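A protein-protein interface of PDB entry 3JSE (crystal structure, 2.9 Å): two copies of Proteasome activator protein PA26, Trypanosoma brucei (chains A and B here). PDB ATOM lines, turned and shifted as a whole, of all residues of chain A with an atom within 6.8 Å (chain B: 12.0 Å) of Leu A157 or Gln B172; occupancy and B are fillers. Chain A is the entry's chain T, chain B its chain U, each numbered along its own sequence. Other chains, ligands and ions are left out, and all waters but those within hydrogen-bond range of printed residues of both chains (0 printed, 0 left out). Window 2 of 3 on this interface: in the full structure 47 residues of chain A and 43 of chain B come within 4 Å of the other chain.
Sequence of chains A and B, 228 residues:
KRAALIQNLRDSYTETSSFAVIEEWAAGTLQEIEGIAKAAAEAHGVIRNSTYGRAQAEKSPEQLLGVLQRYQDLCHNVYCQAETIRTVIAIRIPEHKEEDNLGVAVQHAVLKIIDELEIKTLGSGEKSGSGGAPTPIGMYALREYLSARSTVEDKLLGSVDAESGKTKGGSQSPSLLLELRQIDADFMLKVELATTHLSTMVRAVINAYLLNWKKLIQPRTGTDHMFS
Leu A157 touches just one residue of chain B: Gln B172 (3.4 Å).
Gln B172 touches just one residue of chain A: Leu A157.
No residue of chain B comes within 4 Å of Arg A54.
Ala A57 touches one residue of chain B.
Glu A153 touches just these residues of chain B: Ser B173, Pro B174 and Ser B175.
No residue of chain B comes within 4 Å of Leu A156.
No residue of chain B comes within 4 Å of Ser A171.
Of the printed residues of chain A, Ser B175 touches Glu A153 (2.4 Å).
Printed residues of chain A within 4 Å of Ser B171: Asp A154.
Of the printed residues of chain A, Pro B174 touches Ala A57, Glu A58 and Glu A153.
Printed residues of chain A within 4 Å of Ser B173: Glu A153 (2.5 Å) and Asp A154 (3.1 Å).
The nearest residue of chain B that does not touch Leu A157 is Ser B173 (4.2 Å).
The nearest residue of chain A that does not touch Gln B172 is Asp A154 (4.6 Å).
The nearest printed residue of chain A that does not touch Ser B173 is Leu A157 (4.2 Å).
O of Ala A57 touches CD of Pro B174, at 3.2 Å.
CG of Pro B174 touches C of Glu A58 (3.7 Å).
Ser B173 touches Asp A154.
Gln B172 touches Leu A157.
The guanidinium group (NH2) of Arg A54 lies within salt-bridge range of the side-chain carboxylate (OE2) of Glu A58 (3.4 Å).
The guanidinium group of Arg A54 is in hydrogen-bond range of the backbone carbonyl oxygen of Leu A157 (3.5 Å).
O of Lys B155 lies within hydrogen-bond range of N of Ser B171, 2.8 Å away.
The backbone NH of Ser B173 is in hydrogen-bond range of the side-chain hydroxyl of Ser B171.
OG of Ser B173 sits at hydrogen-bond distance from N of Leu B176, at 3.2 Å.
The side-chain carboxylate of Glu A153 sits at hydrogen-bond distance from the side-chain hydroxyl of Ser B173 (2.5 Å).
The side-chain carboxylate (OE1) of Glu A153 lies within hydrogen-bond range of the backbone NH (N) of Ser B175.
OG of Ser B171 is in hydrogen-bond range of OD1 of Asp A154 (2.5 Å).
OE1 of Glu A153 lies close to N of Pro B174 (3.3 Å).
Asp A154 touches Ser B171, but with the chains exchanged Ser A171 does not touch Asp B154 (18.8 Å).
Of the 8 pairs that touch across the chains among the printed residues, none has its exchanged pair printed and touching as well.
Printed residues of chain A that touch a printed residue of chain B: Ala A57, Glu A58, Glu A153, Asp A154 and Leu A157.
Among the printed residues, 8 pairs touch across the chains.
Among the printed residues, no Asp or Glu carboxylate lies within 4 Å of a Lys or Arg side-chain nitrogen of the other chain.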
ATOM      1  N   ARG A  54      35.295   5.837   3.511  1.00  0.00           N
ATOM      2  CA  ARG A  54      34.136   6.478   2.887  1.00  0.00           C
ATOM      3  C   ARG A  54      32.980   6.659   3.884  1.00  0.00           C
ATOM      4  O   ARG A  54      32.159   7.567   3.740  1.00  0.00           O
ATOM      5  CB  ARG A  54      33.672   5.652   1.675  1.00  0.00           C
ATOM      6  CG  ARG A  54      33.660   6.396   0.331  1.00  0.00           C
ATOM      7  CD  ARG A  54      32.937   5.568  -0.732  1.00  0.00           C
ATOM      8  NE  ARG A  54      31.491   5.558  -0.484  1.00  0.00           N
ATOM      9  CZ  ARG A  54      30.550   5.987  -1.327  1.00  0.00           C
ATOM     10  NH1 ARG A  54      30.864   6.459  -2.541  1.00  0.00           N
ATOM     11  NH2 ARG A  54      29.267   5.936  -0.957  1.00  0.00           N
ATOM     12  N   ALA A  55      32.930   5.797   4.891  1.00  0.00           N
ATOM     13  CA  ALA A  55      31.993   5.942   6.000  1.00  0.00           C
ATOM     14  C   ALA A  55      31.954   7.359   6.549  1.00  0.00           C
ATOM     15  O   ALA A  55      30.894   7.822   6.960  1.00  0.00           O
ATOM     16  CB  ALA A  55      32.353   4.964   7.126  1.00  0.00           C
ATOM     17  N   ALA A  57      32.580  10.173   4.935  1.00  0.00           N
ATOM     18  CA  ALA A  57      31.994  11.144   4.002  1.00  0.00           C
ATOM     19  C   ALA A  57      30.461  11.081   4.040  1.00  0.00           C
ATOM     20  O   ALA A  57      29.788  11.854   3.352  1.00  0.00           O
ATOM     21  CB  ALA A  57      32.501  10.913   2.586  1.00  0.00           C
ATOM     22  N   GLU A  58      29.921  10.178   4.861  1.00  0.00           N
ATOM     23  CA  GLU A  58      28.486   9.942   4.928  1.00  0.00           C
ATOM     24  C   GLU A  58      27.785  10.526   6.149  1.00  0.00           C
ATOM     25  O   GLU A  58      26.578  10.587   6.153  1.00  0.00           O
ATOM     26  CB  GLU A  58      28.208   8.444   4.859  1.00  0.00           C
ATOM     27  CG  GLU A  58      28.666   7.793   3.554  1.00  0.00           C
ATOM     28  CD  GLU A  58      28.378   6.297   3.481  1.00  0.00           C
ATOM     29  OE1 GLU A  58      28.021   5.704   4.511  1.00  0.00           O
ATOM     30  OE2 GLU A  58      28.525   5.713   2.387  1.00  0.00           O
ATOM     31  N   VAL A 152      34.478  18.193  -0.588  1.00  0.00           N
ATOM     32  CA  VAL A 152      35.205  16.926  -0.507  1.00  0.00           C
ATOM     33  C   VAL A 152      34.222  15.736  -0.413  1.00  0.00           C
ATOM     34  O   VAL A 152      34.436  14.682  -1.034  1.00  0.00           O
ATOM     35  CB  VAL A 152      36.247  16.930   0.686  1.00  0.00           C
ATOM     36  CG1 VAL A 152      36.638  15.527   1.111  1.00  0.00           C
ATOM     37  CG2 VAL A 152      37.505  17.696   0.305  1.00  0.00           C
ATOM     38  N   GLU A 153      33.140  15.904   0.346  1.00  0.00           N
ATOM     39  CA  GLU A 153      32.105  14.858   0.455  1.00  0.00           C
ATOM     40  C   GLU A 153      31.480  14.456  -0.888  1.00  0.00           C
ATOM     41  O   GLU A 153      31.354  13.276  -1.181  1.00  0.00           O
ATOM     42  CB  GLU A 153      30.996  15.289   1.411  1.00  0.00           C
ATOM     43  CG  GLU A 153      31.397  15.217   2.875  1.00  0.00           C
ATOM     44  CD  GLU A 153      30.380  15.876   3.784  1.00  0.00           C
ATOM     45  OE1 GLU A 153      29.292  16.227   3.285  1.00  0.00           O
ATOM     46  OE2 GLU A 153      30.674  16.036   4.995  1.00  0.00           O
ATOM     47  N   ASP A 154      31.087  15.436  -1.691  1.00  0.00           N
ATOM     48  CA  ASP A 154      30.616  15.182  -3.062  1.00  0.00           C
ATOM     49  C   ASP A 154      31.599  14.425  -3.919  1.00  0.00           C
ATOM     50  O   ASP A 154      31.237  13.412  -4.483  1.00  0.00           O
ATOM     51  CB  ASP A 154      30.287  16.485  -3.786  1.00  0.00           C
ATOM     52  CG  ASP A 154      28.821  16.810  -3.759  1.00  0.00           C
ATOM     53  OD1 ASP A 154      28.168  16.547  -2.740  1.00  0.00           O
ATOM     54  OD2 ASP A 154      28.323  17.347  -4.761  1.00  0.00           O
ATOM     55  N   LYS A 155      32.832  14.915  -4.030  1.00  0.00           N
ATOM     56  CA  LYS A 155      33.844  14.233  -4.844  1.00  0.00           C
ATOM     57  C   LYS A 155      34.032  12.785  -4.394  1.00  0.00           C
ATOM     58  O   LYS A 155      34.263  11.923  -5.230  1.00  0.00           O
ATOM     59  CB  LYS A 155      35.189  14.969  -4.811  1.00  0.00           C
ATOM     60  CG  LYS A 155      35.178  16.318  -5.506  1.00  0.00           C
ATOM     61  CD  LYS A 155      36.519  17.073  -5.421  1.00  0.00           C
ATOM     62  CE  LYS A 155      36.407  18.455  -6.072  1.00  0.00           C
ATOM     63  NZ  LYS A 155      37.663  18.892  -6.712  1.00  0.00           N
ATOM     64  N   LEU A 156      33.941  12.528  -3.085  1.00  0.00           N
ATOM     65  CA  LEU A 156      34.162  11.170  -2.543  1.00  0.00           C
ATOM     66  C   LEU A 156      32.946  10.227  -2.754  1.00  0.00           C
ATOM     67  O   LEU A 156      33.122   9.013  -2.946  1.00  0.00           O
ATOM     68  CB  LEU A 156      34.539  11.213  -1.048  1.00  0.00           C
ATOM     69  CG  LEU A 156      35.963  11.603  -0.636  1.00  0.00           C
ATOM     70  CD1 LEU A 156      36.015  11.804   0.886  1.00  0.00           C
ATOM     71  CD2 LEU A 156      37.033  10.616  -1.079  1.00  0.00           C
ATOM     72  N   LEU A 157      31.727  10.779  -2.698  1.00  0.00           N
ATOM     73  CA  LEU A 157      30.495   9.985  -2.861  1.00  0.00           C
ATOM     74  C   LEU A 157      30.036   9.906  -4.331  1.00  0.00           C
ATOM     75  O   LEU A 157      29.726   8.850  -4.825  1.00  0.00           O
ATOM     76  CB  LEU A 157      29.350  10.560  -2.002  1.00  0.00           C
ATOM     77  CG  LEU A 157      29.468  10.675  -0.481  1.00  0.00           C
ATOM     78  CD1 LEU A 157      28.273  11.432   0.050  1.00  0.00           C
ATOM     79  CD2 LEU A 157      29.561   9.311   0.193  1.00  0.00           C
ATOM     80  N   GLY A 158      29.990  11.036  -5.020  1.00  0.00           N
ATOM     81  CA  GLY A 158      29.466  11.093  -6.384  1.00  0.00           C
ATOM     82  C   GLY A 158      27.996  11.456  -6.392  1.00  0.00           C
ATOM     83  O   GLY A 158      27.317  11.280  -7.408  1.00  0.00           O
ATOM     84  N   GLY A 169      30.043   7.018  -9.245  1.00  0.00           N
ATOM     85  CA  GLY A 169      31.437   6.716  -8.927  1.00  0.00           C
ATOM     86  C   GLY A 169      32.134   7.801  -8.106  1.00  0.00           C
ATOM     87  O   GLY A 169      32.377   8.915  -8.611  1.00  0.00           O
ATOM     88  N   GLY A 170      32.459   7.480  -6.847  1.00  0.00           N
ATOM     89  CA  GLY A 170      33.248   8.379  -5.994  1.00  0.00           C
ATOM     90  C   GLY A 170      34.720   8.404  -6.377  1.00  0.00           C
ATOM     91  O   GLY A 170      35.237   7.413  -6.909  1.00  0.00           O
ATOM     92  N   SER A 171      35.395   9.526  -6.102  1.00  0.00           N
ATOM     93  CA  SER A 171      36.807   9.695  -6.478  1.00  0.00           C
ATOM     94  C   SER A 171      37.670   8.622  -5.808  1.00  0.00           C
ATOM     95  O   SER A 171      37.390   8.218  -4.687  1.00  0.00           O
ATOM     96  CB  SER A 171      37.316  11.101  -6.110  1.00  0.00           C
ATOM     97  OG  SER A 171      38.725  11.224  -6.311  1.00  0.00           O
ATOM     98  N   TYR B  52      17.472  19.685   9.357  1.00  0.00           N
ATOM     99  CA  TYR B  52      17.117  20.024   7.993  1.00  0.00           C
ATOM    100  C   TYR B  52      17.168  18.762   7.150  1.00  0.00           C
ATOM    101  O   TYR B  52      18.134  18.019   7.205  1.00  0.00           O
ATOM    102  CB  TYR B  52      18.084  21.082   7.438  1.00  0.00           C
ATOM    103  CG  TYR B  52      17.658  22.531   7.615  1.00  0.00           C
ATOM    104  CD1 TYR B  52      17.106  22.993   8.802  1.00  0.00           C
ATOM    105  CD2 TYR B  52      17.853  23.453   6.591  1.00  0.00           C
ATOM    106  CE1 TYR B  52      16.728  24.332   8.944  1.00  0.00           C
ATOM    107  CE2 TYR B  52      17.490  24.789   6.736  1.00  0.00           C
ATOM    108  CZ  TYR B  52      16.938  25.211   7.899  1.00  0.00           C
ATOM    109  OH  TYR B  52      16.604  26.514   7.991  1.00  0.00           O
ATOM    110  N   GLY B  53      16.101  18.521   6.405  1.00  0.00           N
ATOM    111  CA  GLY B  53      16.075  17.521   5.357  1.00  0.00           C
ATOM    112  C   GLY B  53      15.819  18.210   4.041  1.00  0.00           C
ATOM    113  O   GLY B  53      15.747  19.428   3.969  1.00  0.00           O
ATOM    114  N   ARG B  54      15.658  17.412   3.004  1.00  0.00           N
ATOM    115  CA  ARG B  54      15.442  17.919   1.662  1.00  0.00           C
ATOM    116  C   ARG B  54      14.172  18.782   1.592  1.00  0.00           C
ATOM    117  O   ARG B  54      14.092  19.671   0.782  1.00  0.00           O
ATOM    118  CB  ARG B  54      15.348  16.747   0.671  1.00  0.00           C
ATOM    119  CG  ARG B  54      16.380  16.737  -0.448  1.00  0.00           C
ATOM    120  CD  ARG B  54      16.020  15.680  -1.508  1.00  0.00           C
ATOM    121  NE  ARG B  54      14.851  16.107  -2.302  1.00  0.00           N
ATOM    122  CZ  ARG B  54      14.827  16.283  -3.631  1.00  0.00           C
ATOM    123  NH1 ARG B  54      15.911  16.046  -4.386  1.00  0.00           N
ATOM    124  NH2 ARG B  54      13.700  16.697  -4.223  1.00  0.00           N
ATOM    125  N   ALA B  57      14.972  22.397   1.246  1.00  0.00           N
ATOM    126  CA  ALA B  57      15.493  22.943  -0.008  1.00  0.00           C
ATOM    127  C   ALA B  57      14.338  23.286  -0.964  1.00  0.00           C
ATOM    128  O   ALA B  57      14.554  23.879  -2.006  1.00  0.00           O
ATOM    129  CB  ALA B  57      16.497  21.974  -0.650  1.00  0.00           C
ATOM    130  N   THR B 151      22.093  28.386  -4.791  1.00  0.00           N
ATOM    131  CA  THR B 151      23.183  27.498  -5.226  1.00  0.00           C
ATOM    132  C   THR B 151      23.155  26.180  -4.463  1.00  0.00           C
ATOM    133  O   THR B 151      23.280  25.109  -5.064  1.00  0.00           O
ATOM    134  CB  THR B 151      24.581  28.124  -5.082  1.00  0.00           C
ATOM    135  OG1 THR B 151      24.600  29.404  -5.739  1.00  0.00           O
ATOM    136  CG2 THR B 151      25.650  27.197  -5.725  1.00  0.00           C
ATOM    137  N   VAL B 152      22.973  26.258  -3.148  1.00  0.00           N
ATOM    138  CA  VAL B 152      22.840  25.052  -2.334  1.00  0.00           C
ATOM    139  C   VAL B 152      21.535  24.300  -2.667  1.00  0.00           C
ATOM    140  O   VAL B 152      21.528  23.072  -2.731  1.00  0.00           O
ATOM    141  CB  VAL B 152      22.950  25.367  -0.826  1.00  0.00           C
ATOM    142  CG1 VAL B 152      22.369  24.250   0.017  1.00  0.00           C
ATOM    143  CG2 VAL B 152      24.388  25.596  -0.454  1.00  0.00           C
ATOM    144  N   GLU B 153      20.445  25.027  -2.905  1.00  0.00           N
ATOM    145  CA  GLU B 153      19.174  24.389  -3.271  1.00  0.00           C
ATOM    146  C   GLU B 153      19.290  23.529  -4.525  1.00  0.00           C
ATOM    147  O   GLU B 153      18.867  22.373  -4.519  1.00  0.00           O
ATOM    148  CB  GLU B 153      18.063  25.422  -3.429  1.00  0.00           C
ATOM    149  CG  GLU B 153      17.555  25.978  -2.098  1.00  0.00           C
ATOM    150  CD  GLU B 153      16.735  27.241  -2.267  1.00  0.00           C
ATOM    151  OE1 GLU B 153      16.371  27.562  -3.418  1.00  0.00           O
ATOM    152  OE2 GLU B 153      16.455  27.921  -1.255  1.00  0.00           O
ATOM    153  N   ASP B 154      19.875  24.083  -5.583  1.00  0.00           N
ATOM    154  CA  ASP B 154      20.131  23.325  -6.815  1.00  0.00           C
ATOM    155  C   ASP B 154      20.932  22.047  -6.605  1.00  0.00           C
ATOM    156  O   ASP B 154      20.545  20.994  -7.082  1.00  0.00           O
ATOM    157  CB  ASP B 154      20.859  24.188  -7.859  1.00  0.00           C
ATOM    158  CG  ASP B 154      19.913  24.764  -8.920  1.00  0.00           C
ATOM    159  OD1 ASP B 154      18.777  25.166  -8.553  1.00  0.00           O
ATOM    160  OD2 ASP B 154      20.309  24.795 -10.115  1.00  0.00           O
ATOM    161  N   LYS B 155      22.065  22.141  -5.927  1.00  0.00           N
ATOM    162  CA  LYS B 155      22.886  20.956  -5.698  1.00  0.00           C
ATOM    163  C   LYS B 155      22.109  19.896  -4.952  1.00  0.00           C
ATOM    164  O   LYS B 155      22.300  18.726  -5.218  1.00  0.00           O
ATOM    165  CB  LYS B 155      24.171  21.298  -4.943  1.00  0.00           C
ATOM    166  CG  LYS B 155      25.156  22.121  -5.761  1.00  0.00           C
ATOM    167  CD  LYS B 155      26.422  22.510  -4.981  1.00  0.00           C
ATOM    168  CE  LYS B 155      27.338  23.422  -5.835  1.00  0.00           C
ATOM    169  NZ  LYS B 155      28.783  23.143  -5.545  1.00  0.00           N
ATOM    170  N   LEU B 156      21.221  20.309  -4.041  1.00  0.00           N
ATOM    171  CA  LEU B 156      20.435  19.354  -3.204  1.00  0.00           C
ATOM    172  C   LEU B 156      19.244  18.710  -3.940  1.00  0.00           C
ATOM    173  O   LEU B 156      18.896  17.539  -3.662  1.00  0.00           O
ATOM    174  CB  LEU B 156      19.939  20.001  -1.884  1.00  0.00           C
ATOM    175  CG  LEU B 156      20.903  20.198  -0.702  1.00  0.00           C
ATOM    176  CD1 LEU B 156      20.234  21.013   0.350  1.00  0.00           C
ATOM    177  CD2 LEU B 156      21.388  18.915  -0.099  1.00  0.00           C
ATOM    178  N   LEU B 157      18.617  19.470  -4.845  1.00  0.00           N
ATOM    179  CA  LEU B 157      17.465  18.982  -5.610  1.00  0.00           C
ATOM    180  C   LEU B 157      17.869  18.306  -6.939  1.00  0.00           C
ATOM    181  O   LEU B 157      17.424  17.206  -7.220  1.00  0.00           O
ATOM    182  CB  LEU B 157      16.470  20.115  -5.888  1.00  0.00           C
ATOM    183  CG  LEU B 157      15.841  20.909  -4.732  1.00  0.00           C
ATOM    184  CD1 LEU B 157      15.017  22.073  -5.303  1.00  0.00           C
ATOM    185  CD2 LEU B 157      15.006  20.034  -3.814  1.00  0.00           C
ATOM    186  N   GLY B 158      18.711  18.956  -7.740  1.00  0.00           N
ATOM    187  CA  GLY B 158      19.100  18.451  -9.054  1.00  0.00           C
ATOM    188  C   GLY B 158      18.226  19.027 -10.127  1.00  0.00           C
ATOM    189  O   GLY B 158      18.273  18.554 -11.258  1.00  0.00           O
ATOM    190  N   GLY B 169      19.230  13.592  -9.811  1.00  0.00           N
ATOM    191  CA  GLY B 169      19.877  13.135  -8.583  1.00  0.00           C
ATOM    192  C   GLY B 169      20.450  14.278  -7.756  1.00  0.00           C
ATOM    193  O   GLY B 169      21.414  14.921  -8.155  1.00  0.00           O
ATOM    194  N   GLY B 170      19.843  14.541  -6.598  1.00  0.00           N
ATOM    195  CA  GLY B 170      20.357  15.534  -5.669  1.00  0.00           C
ATOM    196  C   GLY B 170      21.621  15.058  -4.976  1.00  0.00           C
ATOM    197  O   GLY B 170      21.826  13.862  -4.828  1.00  0.00           O
ATOM    198  N   SER B 171      22.458  15.997  -4.542  1.00  0.00           N
ATOM    199  CA  SER B 171      23.717  15.667  -3.890  1.00  0.00           C
ATOM    200  C   SER B 171      23.463  14.885  -2.612  1.00  0.00           C
ATOM    201  O   SER B 171      22.500  15.139  -1.918  1.00  0.00           O
ATOM    202  CB  SER B 171      24.526  16.936  -3.592  1.00  0.00           C
ATOM    203  OG  SER B 171      25.663  16.661  -2.782  1.00  0.00           O
ATOM    204  N   GLN B 172      24.345  13.937  -2.327  1.00  0.00           N
ATOM    205  CA  GLN B 172      24.244  13.086  -1.154  1.00  0.00           C
ATOM    206  C   GLN B 172      25.125  13.589   0.007  1.00  0.00           C
ATOM    207  O   GLN B 172      25.299  12.891   0.992  1.00  0.00           O
ATOM    208  CB  GLN B 172      24.656  11.634  -1.540  1.00  0.00           C
ATOM    209  CG  GLN B 172      23.627  10.822  -2.404  1.00  0.00           C
ATOM    210  CD  GLN B 172      22.159  10.794  -1.816  1.00  0.00           C
ATOM    211  OE1 GLN B 172      21.945  10.774  -0.594  1.00  0.00           O
ATOM    212  NE2 GLN B 172      21.163  10.794  -2.705  1.00  0.00           N
ATOM    213  N   SER B 173      25.698  14.787  -0.116  1.00  0.00           N
ATOM    214  CA  SER B 173      26.688  15.278   0.851  1.00  0.00           C
ATOM    215  C   SER B 173      25.996  15.647   2.150  1.00  0.00           C
ATOM    216  O   SER B 173      25.214  16.579   2.162  1.00  0.00           O
ATOM    217  CB  SER B 173      27.464  16.496   0.278  1.00  0.00           C
ATOM    218  OG  SER B 173      28.264  17.155   1.260  1.00  0.00           O
ATOM    219  N   PRO B 174      26.305  14.934   3.248  1.00  0.00           N
ATOM    220  CA  PRO B 174      25.684  15.312   4.522  1.00  0.00           C
ATOM    221  C   PRO B 174      25.938  16.776   4.937  1.00  0.00           C
ATOM    222  O   PRO B 174      25.050  17.413   5.509  1.00  0.00           O
ATOM    223  CB  PRO B 174      26.328  14.347   5.537  1.00  0.00           C
ATOM    224  CG  PRO B 174      27.603  13.960   4.923  1.00  0.00           C
ATOM    225  CD  PRO B 174      27.347  13.908   3.444  1.00  0.00           C
ATOM    226  N   SER B 175      27.132  17.287   4.654  1.00  0.00           N
ATOM    227  CA  SER B 175      27.503  18.630   5.030  1.00  0.00           C
ATOM    228  C   SER B 175      26.788  19.645   4.169  1.00  0.00           C
ATOM    229  O   SER B 175      26.454  20.706   4.671  1.00  0.00           O
ATOM    230  CB  SER B 175      29.011  18.820   4.904  1.00  0.00           C
ATOM    231  OG  SER B 175      29.674  18.020   5.866  1.00  0.00           O
ATOM    232  N   LEU B 176      26.558  19.352   2.887  1.00  0.00           N
ATOM    233  CA  LEU B 176      25.843  20.302   2.036  1.00  0.00           C
ATOM    234  C   LEU B 176      24.472  20.594   2.597  1.00  0.00           C
ATOM    235  O   LEU B 176      23.984  21.717   2.515  1.00  0.00           O
ATOM    236  CB  LEU B 176      25.729  19.821   0.594  1.00  0.00           C
ATOM    237  CG  LEU B 176      25.013  20.780  -0.378  1.00  0.00           C
ATOM    238  CD1 LEU B 176      25.713  22.125  -0.473  1.00  0.00           C
ATOM    239  CD2 LEU B 176      24.876  20.159  -1.757  1.00  0.00           C
ATOM    240  N   LEU B 177      23.858  19.587   3.196  1.00  0.00           N
ATOM    241  CA  LEU B 177      22.560  19.764   3.842  1.00  0.00           C
ATOM    242  C   LEU B 177      22.669  20.651   5.071  1.00  0.00           C
ATOM    243  O   LEU B 177      21.820  21.491   5.310  1.00  0.00           O
ATOM    244  CB  LEU B 177      21.971  18.402   4.228  1.00  0.00           C
ATOM    245  CG  LEU B 177      20.538  18.409   4.781  1.00  0.00           C
ATOM    246  CD1 LEU B 177      19.542  18.878   3.715  1.00  0.00           C
ATOM    247  CD2 LEU B 177      20.205  17.014   5.264  1.00  0.00           C
ATOM    248  N   LEU B 178      23.705  20.438   5.863  1.00  0.00           N
ATOM    249  CA  LEU B 178      23.950  21.261   7.050  1.00  0.00           C
ATOM    250  C   LEU B 178      24.327  22.693   6.684  1.00  0.00           C
ATOM    251  O   LEU B 178      24.107  23.606   7.452  1.00  0.00           O
ATOM    252  CB  LEU B 178      25.050  20.643   7.931  1.00  0.00           C
ATOM    253  CG  LEU B 178      24.742  19.403   8.790  1.00  0.00           C
ATOM    254  CD1 LEU B 178      26.001  18.819   9.330  1.00  0.00           C
ATOM    255  CD2 LEU B 178      23.827  19.696   9.938  1.00  0.00           C
ATOM    256  N   GLU B 179      24.912  22.873   5.505  1.00  0.00           N
ATOM    257  CA  GLU B 179      25.244  24.204   4.970  1.00  0.00           C
ATOM    258  C   GLU B 179      23.965  25.008   4.651  1.00  0.00           C
ATOM    259  O   GLU B 179      23.890  26.188   4.949  1.00  0.00           O
ATOM    260  CB  GLU B 179      26.166  24.097   3.730  1.00  0.00           C
ATOM    261  CG  GLU B 179      26.663  25.463   3.176  1.00  0.00           C
ATOM    262  CD  GLU B 179      27.750  25.374   2.057  1.00  0.00           C
ATOM    263  OE1 GLU B 179      28.386  26.410   1.764  1.00  0.00           O
ATOM    264  OE2 GLU B 179      27.982  24.292   1.468  1.00  0.00           O
ATOM    265  N   LEU B 180      22.963  24.379   4.047  1.00  0.00           N
ATOM    266  CA  LEU B 180      21.691  25.062   3.824  1.00  0.00           C
ATOM    267  C   LEU B 180      21.175  25.643   5.133  1.00  0.00           C
ATOM    268  O   LEU B 180      20.634  26.746   5.160  1.00  0.00           O
ATOM    269  CB  LEU B 180      20.652  24.114   3.256  1.00  0.00           C
ATOM    270  CG  LEU B 180      19.338  24.774   2.890  1.00  0.00           C
ATOM    271  CD1 LEU B 180      19.529  25.753   1.738  1.00  0.00           C
ATOM    272  CD2 LEU B 180      18.355  23.711   2.516  1.00  0.00           C
